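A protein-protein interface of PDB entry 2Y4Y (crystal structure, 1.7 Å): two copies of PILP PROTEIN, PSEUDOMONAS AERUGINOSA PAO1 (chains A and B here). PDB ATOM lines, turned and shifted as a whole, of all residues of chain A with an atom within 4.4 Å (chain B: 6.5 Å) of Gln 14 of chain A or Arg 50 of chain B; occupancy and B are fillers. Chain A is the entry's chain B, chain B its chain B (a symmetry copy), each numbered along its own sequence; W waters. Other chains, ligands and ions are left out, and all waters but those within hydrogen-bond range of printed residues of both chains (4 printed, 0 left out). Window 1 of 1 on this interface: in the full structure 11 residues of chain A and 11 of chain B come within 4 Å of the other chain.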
ATOM      1  N   VAL A  12      16.764  12.541  -2.688  1.00  0.00           N
ATOM      2  CA  VAL A  12      16.082  12.074  -3.964  1.00  0.00           C
ATOM      3  C   VAL A  12      16.395  13.109  -5.109  1.00  0.00           C
ATOM      4  O   VAL A  12      16.073  14.291  -4.955  1.00  0.00           O
ATOM      5  CB  VAL A  12      14.515  11.984  -3.764  1.00  0.00           C
ATOM      6  CG1 VAL A  12      13.792  11.593  -5.054  1.00  0.00           C
ATOM      7  CG2 VAL A  12      14.104  10.989  -2.579  1.00  0.00           C
ATOM      8  N   LYS A  13      17.006  12.647  -6.205  1.00  0.00           N
ATOM      9  CA  LYS A  13      17.475  13.556  -7.252  1.00  0.00           C
ATOM     10  C   LYS A  13      16.316  14.162  -8.052  1.00  0.00           C
ATOM     11  O   LYS A  13      15.181  13.585  -8.147  1.00  0.00           O
ATOM     12  CB  LYS A  13      18.484  12.897  -8.199  1.00  0.00           C
ATOM     13  CG  LYS A  13      19.849  12.381  -7.541  1.00  0.00           C
ATOM     14  CD  LYS A  13      20.788  13.490  -7.004  1.00  0.00           C
ATOM     15  CE  LYS A  13      21.657  14.095  -8.120  1.00  0.00           C
ATOM     16  NZ  LYS A  13      23.036  14.434  -7.769  1.00  0.00           N
ATOM     17  N   GLN A  14      16.580  15.351  -8.634  1.00  0.00           N
ATOM     18  CA  GLN A  14      15.526  16.053  -9.361  1.00  0.00           C
ATOM     19  C   GLN A  14      15.859  15.935 -10.840  1.00  0.00           C
ATOM     20  O   GLN A  14      17.024  15.814 -11.201  1.00  0.00           O
ATOM     21  CB  GLN A  14      15.447  17.496  -8.931  1.00  0.00           C
ATOM     22  CG  GLN A  14      15.018  17.521  -7.480  1.00  0.00           C
ATOM     23  CD  GLN A  14      14.499  18.851  -7.012  1.00  0.00           C
ATOM     24  OE1 GLN A  14      14.851  19.866  -7.547  1.00  0.00           O
ATOM     25  NE2 GLN A  14      13.745  18.856  -5.923  1.00  0.00           N
ATOM     26  N   PHE A  15      14.819  16.017 -11.664  1.00  0.00           N
ATOM     27  CA  PHE A  15      14.989  15.836 -13.133  1.00  0.00           C
ATOM     28  C   PHE A  15      16.012  16.861 -13.666  1.00  0.00           C
ATOM     29  O   PHE A  15      16.842  16.503 -14.502  1.00  0.00           O
ATOM     30  CB  PHE A  15      13.598  16.078 -13.809  1.00  0.00           C
ATOM     31  CG  PHE A  15      13.679  16.159 -15.337  1.00  0.00           C
ATOM     32  CD1 PHE A  15      14.042  15.010 -16.060  1.00  0.00           C
ATOM     33  CD2 PHE A  15      13.403  17.347 -16.007  1.00  0.00           C
ATOM     34  CE1 PHE A  15      14.153  15.081 -17.533  1.00  0.00           C
ATOM     35  CE2 PHE A  15      13.504  17.413 -17.505  1.00  0.00           C
ATOM     36  CZ  PHE A  15      13.904  16.290 -18.177  1.00  0.00           C
ATOM     37  N   LEU A  16      15.926  18.127 -13.213  1.00  0.00           N
ATOM     38  CA  LEU A  16      16.838  19.148 -13.804  1.00  0.00           C
ATOM     39  C   LEU A  16      18.293  19.003 -13.352  1.00  0.00           C
ATOM     40  O   LEU A  16      19.131  19.784 -13.807  1.00  0.00           O
ATOM     41  CB  LEU A  16      16.296  20.577 -13.536  1.00  0.00           C
ATOM     42  CG  LEU A  16      14.885  20.791 -14.100  1.00  0.00           C
ATOM     43  CD1 LEU A  16      14.414  22.184 -13.673  1.00  0.00           C
ATOM     44  CD2 LEU A  16      14.995  20.810 -15.634  1.00  0.00           C
ATOM     45  N   GLU A  17      18.602  17.985 -12.554  1.00  0.00           N
ATOM     46  CA  GLU A  17      20.029  17.676 -12.278  1.00  0.00           C
ATOM     47  C   GLU A  17      20.665  16.851 -13.405  1.00  0.00           C
ATOM     48  O   GLU A  17      21.870  16.539 -13.375  1.00  0.00           O
ATOM     49  CB  GLU A  17      20.127  16.905 -10.942  1.00  0.00           C
ATOM     50  CG  GLU A  17      19.638  17.803  -9.816  1.00  0.00           C
ATOM     51  CD  GLU A  17      19.892  17.160  -8.482  1.00  0.00           C
ATOM     52  OE1 GLU A  17      21.081  17.181  -8.014  1.00  0.00           O
ATOM     53  OE2 GLU A  17      18.891  16.711  -7.902  1.00  0.00           O
ATOM     54  N   GLY A  18      19.862  16.428 -14.415  1.00  0.00           N
ATOM     55  CA  GLY A  18      20.429  15.614 -15.507  1.00  0.00           C
ATOM     56  C   GLY A  18      20.828  16.474 -16.736  1.00  0.00           C
ATOM     57  O   GLY A  18      20.761  15.989 -17.910  1.00  0.00           O
ATOM     58  N   ASP A  53      14.910  23.602  -4.620  1.00  0.00           N
ATOM     59  CA  ASP A  53      15.046  22.668  -5.729  1.00  0.00           C
ATOM     60  C   ASP A  53      16.476  22.693  -6.314  1.00  0.00           C
ATOM     61  O   ASP A  53      17.320  23.561  -5.949  1.00  0.00           O
ATOM     62  CB  ASP A  53      14.034  23.029  -6.844  1.00  0.00           C
ATOM     63  CG  ASP A  53      12.579  22.686  -6.465  1.00  0.00           C
ATOM     64  OD1 ASP A  53      12.453  21.850  -5.527  1.00  0.00           O
ATOM     65  OD2 ASP A  53      11.626  23.249  -7.127  1.00  0.00           O
ATOM     66  N   TYR A  54      16.773  21.826  -7.285  1.00  0.00           N
ATOM     67  CA  TYR A  54      18.192  21.770  -7.739  1.00  0.00           C
ATOM     68  C   TYR A  54      18.285  21.899  -9.250  1.00  0.00           C
ATOM     69  O   TYR A  54      17.365  21.499 -10.007  1.00  0.00           O
ATOM     70  CB  TYR A  54      18.777  20.413  -7.346  1.00  0.00           C
ATOM     71  CG  TYR A  54      19.070  20.276  -5.867  1.00  0.00           C
ATOM     72  CD1 TYR A  54      18.014  20.010  -4.941  1.00  0.00           C
ATOM     73  CD2 TYR A  54      20.388  20.367  -5.429  1.00  0.00           C
ATOM     74  CE1 TYR A  54      18.311  19.878  -3.584  1.00  0.00           C
ATOM     75  CE2 TYR A  54      20.686  20.216  -4.099  1.00  0.00           C
ATOM     76  CZ  TYR A  54      19.659  19.996  -3.197  1.00  0.00           C
ATOM     77  OH  TYR A  54      19.990  19.927  -1.867  1.00  0.00           O
ATOM     78  N   GLN B  14       3.702  22.299  -4.544  1.00  0.00           N
ATOM     79  CA  GLN B  14       4.399  22.110  -5.813  1.00  0.00           C
ATOM     80  C   GLN B  14       3.612  22.877  -6.865  1.00  0.00           C
ATOM     81  O   GLN B  14       2.408  23.055  -6.725  1.00  0.00           O
ATOM     82  CB  GLN B  14       4.493  20.646  -6.161  1.00  0.00           C
ATOM     83  CG  GLN B  14       5.368  19.981  -5.121  1.00  0.00           C
ATOM     84  CD  GLN B  14       5.897  18.635  -5.528  1.00  0.00           C
ATOM     85  OE1 GLN B  14       5.306  17.963  -6.327  1.00  0.00           O
ATOM     86  NE2 GLN B  14       6.962  18.185  -4.880  1.00  0.00           N
ATOM     87  N   GLN B  34      18.696  10.045 -12.922  1.00  0.00           N
ATOM     88  CA  GLN B  34      18.044  10.746 -11.838  1.00  0.00           C
ATOM     89  C   GLN B  34      16.807  10.016 -11.259  1.00  0.00           C
ATOM     90  O   GLN B  34      16.344  10.397 -10.188  1.00  0.00           O
ATOM     91  CB  GLN B  34      17.613  12.145 -12.245  1.00  0.00           C
ATOM     92  CG  GLN B  34      18.805  13.085 -12.312  1.00  0.00           C
ATOM     93  CD  GLN B  34      19.743  12.793 -13.431  1.00  0.00           C
ATOM     94  OE1 GLN B  34      19.329  12.662 -14.578  1.00  0.00           O
ATOM     95  NE2 GLN B  34      21.080  12.735 -13.119  1.00  0.00           N
ATOM     96  N   THR B  36      13.070   7.598 -12.146  1.00  0.00           N
ATOM     97  CA  THR B  36      11.903   7.231 -12.999  1.00  0.00           C
ATOM     98  C   THR B  36      10.888   8.360 -12.899  1.00  0.00           C
ATOM     99  O   THR B  36      10.494   8.761 -11.804  1.00  0.00           O
ATOM    100  CB  THR B  36      11.352   5.910 -12.485  1.00  0.00           C
ATOM    101  OG1 THR B  36      12.303   4.881 -12.808  1.00  0.00           O
ATOM    102  CG2 THR B  36       9.987   5.604 -13.246  1.00  0.00           C
ATOM    103  N   PHE B  37      10.459   8.985 -13.959  1.00  0.00           N
ATOM    104  CA  PHE B  37       9.556  10.097 -13.924  1.00  0.00           C
ATOM    105  C   PHE B  37       8.381   9.753 -14.817  1.00  0.00           C
ATOM    106  O   PHE B  37       8.590   9.187 -15.916  1.00  0.00           O
ATOM    107  CB  PHE B  37      10.237  11.341 -14.564  1.00  0.00           C
ATOM    108  CG  PHE B  37      11.471  11.752 -13.829  1.00  0.00           C
ATOM    109  CD1 PHE B  37      11.368  12.645 -12.751  1.00  0.00           C
ATOM    110  CD2 PHE B  37      12.704  11.220 -14.198  1.00  0.00           C
ATOM    111  CE1 PHE B  37      12.558  13.001 -12.020  1.00  0.00           C
ATOM    112  CE2 PHE B  37      13.879  11.547 -13.443  1.00  0.00           C
ATOM    113  CZ  PHE B  37      13.772  12.484 -12.397  1.00  0.00           C
ATOM    114  N   ALA B  38       7.179  10.211 -14.444  1.00  0.00           N
ATOM    115  CA  ALA B  38       6.056  10.107 -15.399  1.00  0.00           C
ATOM    116  C   ALA B  38       6.093  11.373 -16.188  1.00  0.00           C
ATOM    117  O   ALA B  38       6.400  12.406 -15.629  1.00  0.00           O
ATOM    118  CB  ALA B  38       4.779  10.089 -14.600  1.00  0.00           C
ATOM    119  N   ARG B  48       7.976  16.407 -15.808  1.00  0.00           N
ATOM    120  CA  ARG B  48       8.508  15.132 -15.344  1.00  0.00           C
ATOM    121  C   ARG B  48       8.190  15.024 -13.845  1.00  0.00           C
ATOM    122  O   ARG B  48       8.658  15.886 -13.090  1.00  0.00           O
ATOM    123  CB  ARG B  48      10.026  15.148 -15.464  1.00  0.00           C
ATOM    124  CG  ARG B  48      10.556  15.270 -16.794  1.00  0.00           C
ATOM    125  CD  ARG B  48      10.628  14.198 -17.610  1.00  0.00           C
ATOM    126  NE  ARG B  48      10.727  14.762 -19.034  1.00  0.00           N
ATOM    127  CZ  ARG B  48      10.609  16.036 -19.356  1.00  0.00           C
ATOM    128  NH1 ARG B  48      10.368  16.944 -18.389  1.00  0.00           N
ATOM    129  NH2 ARG B  48      10.689  16.417 -20.635  1.00  0.00           N
ATOM    130  N   VAL B  49       7.405  14.025 -13.417  1.00  0.00           N
ATOM    131  CA  VAL B  49       6.899  13.939 -12.042  1.00  0.00           C
ATOM    132  C   VAL B  49       7.376  12.622 -11.442  1.00  0.00           C
ATOM    133  O   VAL B  49       7.376  11.587 -12.105  1.00  0.00           O
ATOM    134  CB  VAL B  49       5.379  13.939 -12.081  1.00  0.00           C
ATOM    135  CG1 VAL B  49       4.861  13.982 -10.772  1.00  0.00           C
ATOM    136  CG2 VAL B  49       4.923  15.200 -12.924  1.00  0.00           C
ATOM    137  N   ARG B  50       7.817  12.661 -10.167  1.00  0.00           N
ATOM    138  CA  ARG B  50       8.414  11.447  -9.510  1.00  0.00           C
ATOM    139  C   ARG B  50       7.374  10.906  -8.516  1.00  0.00           C
ATOM    140  O   ARG B  50       6.463  11.640  -8.087  1.00  0.00           O
ATOM    141  CB  ARG B  50       9.617  11.922  -8.580  1.00  0.00           C
ATOM    142  CG  ARG B  50      10.674  12.661  -9.327  1.00  0.00           C
ATOM    143  CD  ARG B  50      11.689  13.386  -8.432  1.00  0.00           C
ATOM    144  NE  ARG B  50      11.083  14.506  -7.708  1.00  0.00           N
ATOM    145  CZ  ARG B  50      11.623  15.147  -6.675  1.00  0.00           C
ATOM    146  NH1 ARG B  50      12.885  14.857  -6.216  1.00  0.00           N
ATOM    147  NH2 ARG B  50      10.908  16.093  -6.122  1.00  0.00           N
ATOM    148  N   VAL B  51       7.575   9.675  -8.044  1.00  0.00           N
ATOM    149  CA  VAL B  51       6.810   9.223  -6.837  1.00  0.00           C
ATOM    150  C   VAL B  51       7.137  10.179  -5.689  1.00  0.00           C
ATOM    151  O   VAL B  51       8.313  10.541  -5.451  1.00  0.00           O
ATOM    152  CB  VAL B  51       7.184   7.778  -6.542  1.00  0.00           C
ATOM    153  CG1 VAL B  51       6.691   7.220  -5.175  1.00  0.00           C
ATOM    154  CG2 VAL B  51       6.663   6.855  -7.635  1.00  0.00           C
ATOM    155  N   GLY B  52       6.065  10.636  -5.048  1.00  0.00           N
ATOM    156  CA  GLY B  52       6.149  11.565  -3.917  1.00  0.00           C
ATOM    157  C   GLY B  52       5.968  13.020  -4.331  1.00  0.00           C
ATOM    158  O   GLY B  52       5.853  13.883  -3.468  1.00  0.00           O
ATOM    159  N   ASP B  53       5.893  13.302  -5.649  1.00  0.00           N
ATOM    160  CA  ASP B  53       5.481  14.630  -6.080  1.00  0.00           C
ATOM    161  C   ASP B  53       3.942  14.763  -6.106  1.00  0.00           C
ATOM    162  O   ASP B  53       3.193  13.757  -5.936  1.00  0.00           O
ATOM    163  CB  ASP B  53       6.041  14.919  -7.494  1.00  0.00           C
ATOM    164  CG  ASP B  53       7.563  15.165  -7.497  1.00  0.00           C
ATOM    165  OD1 ASP B  53       8.058  15.474  -6.377  1.00  0.00           O
ATOM    166  OD2 ASP B  53       8.197  15.059  -8.616  1.00  0.00           O
ATOM    167  N   TYR B  54       3.418  15.955  -6.401  1.00  0.00           N
ATOM    168  CA  TYR B  54       1.938  16.097  -6.285  1.00  0.00           C
ATOM    169  C   TYR B  54       1.348  16.683  -7.556  1.00  0.00           C
ATOM    170  O   TYR B  54       2.000  17.465  -8.291  1.00  0.00           O
ATOM    171  CB  TYR B  54       1.630  17.058  -5.137  1.00  0.00           C
ATOM    172  CG  TYR B  54       1.847  16.463  -3.762  1.00  0.00           C
ATOM    173  CD1 TYR B  54       3.166  16.353  -3.222  1.00  0.00           C
ATOM    174  CD2 TYR B  54       0.742  16.068  -3.015  1.00  0.00           C
ATOM    175  CE1 TYR B  54       3.340  15.809  -1.948  1.00  0.00           C
ATOM    176  CE2 TYR B  54       0.908  15.554  -1.755  1.00  0.00           C
ATOM    177  CZ  TYR B  54       2.187  15.411  -1.246  1.00  0.00           C
ATOM    178  OH  TYR B  54       2.315  14.823  -0.013  1.00  0.00           O
ATOM    179  N   VAL B  62       1.686  11.462  -5.870  1.00  0.00           N
ATOM    180  CA  VAL B  62       1.990  10.350  -6.808  1.00  0.00           C
ATOM    181  C   VAL B  62       2.619   9.205  -5.983  1.00  0.00           C
ATOM    182  O   VAL B  62       3.601   9.399  -5.281  1.00  0.00           O
ATOM    183  CB  VAL B  62       3.022  10.808  -7.890  1.00  0.00           C
ATOM    184  CG1 VAL B  62       3.384   9.630  -8.757  1.00  0.00           C
ATOM    185  CG2 VAL B  62       2.355  11.861  -8.718  1.00  0.00           C
ATOM    186  N   VAL B  63       1.960   8.027  -5.981  1.00  0.00           N
ATOM    187  CA  VAL B  63       2.472   6.883  -5.232  1.00  0.00           C
ATOM    188  C   VAL B  63       3.005   5.764  -6.059  1.00  0.00           C
ATOM    189  O   VAL B  63       3.627   4.839  -5.565  1.00  0.00           O
ATOM    190  CB  VAL B  63       1.359   6.355  -4.264  1.00  0.00           C
ATOM    191  CG1 VAL B  63       0.966   7.449  -3.279  1.00  0.00           C
ATOM    192  CG2 VAL B  63       0.123   5.844  -5.071  1.00  0.00           C
ATOM    193  N   ILE B  65       4.391   4.730 -10.318  1.00  0.00           N
ATOM    194  CA  ILE B  65       4.509   4.943 -11.772  1.00  0.00           C
ATOM    195  C   ILE B  65       4.885   3.640 -12.399  1.00  0.00           C
ATOM    196  O   ILE B  65       5.960   3.119 -12.129  1.00  0.00           O
ATOM    197  CB  ILE B  65       5.628   6.022 -12.027  1.00  0.00           C
ATOM    198  CG1 ILE B  65       5.215   7.359 -11.415  1.00  0.00           C
ATOM    199  CG2 ILE B  65       5.851   6.244 -13.556  1.00  0.00           C
ATOM    200  CD1 ILE B  65       6.411   8.388 -11.394  1.00  0.00           C
HETATM  201  O   HOH W   1      17.224  13.981 -15.710  1.00  0.00           O
HETATM  202  O   HOH W   2      22.021  12.946 -10.623  1.00  0.00           O
HETATM  203  O   HOH W   3      14.298  10.852  -8.566  1.00  0.00           O
HETATM  204  O   HOH W   4      12.332  16.343 -10.385  1.00  0.00           O
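O of Val 12 of chain A sits at hydrogen-bond distance from NH1 of Arg 50 of chain B, 3.5 Å away.
O of Lys 13 of chain A sits at hydrogen-bond distance from NH1 of Arg 50 of chain B (3.3 Å).
The side-chain amino group (NZ) of Lys 13 of chain A is in salt-bridge range of the side-chain carboxylate (OE1) of Glu 17 of chain A.
N of Gln 14 of chain A lies within hydrogen-bond range of OE2 of Glu 17 of chain A (2.8 Å).
The side-chain carboxylate (OD1) of Asp 53 of chain A is in hydrogen-bond range of the side-chain amide nitrogen (NE2) of Gln 14 of chain A, at 3.3 Å.
The side-chain amide oxygen of Gln 14 of chain A is in hydrogen-bond range of the backbone NH of Tyr 54 of chain A, at 2.8 Å.
The guanidinium group (NH2) of Arg 50 of chain B is in salt-bridge range of the side-chain carboxylate (OD1) of Asp 53 of chain B.
Among the printed residues, merely in contact across the chains: Gly 18 of chain A with Gln 34 of chain B (3.3 Å), Phe 15 of chain A with Arg 48 of chain B (3.3 Å), Gln 14 of chain A with Gln 34 of chain B (3.4 Å), Gln 14 of chain A with Arg 50 of chain B (3.6 Å), Phe 15 of chain A with Phe 37 of chain B (3.6 Å), Lys 13 of chain A with Gln 34 of chain B (3.8 Å) and Glu 17 of chain A with Gln 34 of chain B (3.9 Å).
Gln 14 of chain A touches just these residues of chain B: Gln 34 and Arg 50.
Arg 50 of chain B touches just these residues of chain A: Val 12 (3.5 Å), Lys 13 (3.3 Å) and Gln 14 (3.6 Å).
Of the printed residues of chain B, Phe 15 of chain A touches Phe 37 and Arg 48.
Of the printed residues of chain B, Val 12 of chain A touches Arg 50 (3.5 Å).
Of the printed residues of chain A, Gln 34 of chain B touches Lys 13 (3.8 Å), Gln 14 (3.4 Å), Glu 17 (3.9 Å) and Gly 18 (3.3 Å).
Of the printed residues of chain A, Phe 37 of chain B touches Phe 15.
Printed residues of chain B within 4 Å of Gly 18 of chain A: Gln 34 (3.3 Å).
Ile 65 of chain B touches none of the printed residues of chain A.
The nearest residue of chain B that does not touch Gln 14 of chain A is Phe 37 of chain B (4.3 Å).
The nearest printed residue of chain A that does not touch Arg 50 of chain B is Phe 15 of chain A (5.2 Å).
Printed residues of chain B that touch a printed residue of chain A: Gln 34, Phe 37, Arg 48 and Arg 50.
Hydrophobic or aromatic side chains of chain B within 4 Å of the printed part of chain A: Phe 37.
Of the 9 printed residues of chain A, 6 touch a printed residue of chain B.
Among the printed residues, 9 pairs touch across the chains.
Among the printed residues, no Asp or Glu carboxylate lies within 4 Å of a Lys or Arg side-chain nitrogen of the other chain.
3 positions are printed for both chains.
Water W3 bridges the backbone carbonyl oxygen of Gln 34 of chain B (2.7 Å) and the backbone carbonyl oxygen of Lys 13 of chain A (2.9 Å).
Water W2 lies within hydrogen-bond range of the side-chain amide nitrogen of Gln 34 of chain B (2.7 Å) and the side-chain amino group of Lys 13 of chain A (3.4 Å).
Water W1 lies within hydrogen-bond range of OE1 of Gln 34 of chain B (2.7 Å) and O of Phe 15 of chain A (2.8 Å).
Water W4 bridges the backbone NH of Phe 15 of chain A (2.8 Å) and the guanidinium group of Arg 50 of chain B (3.5 Å).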
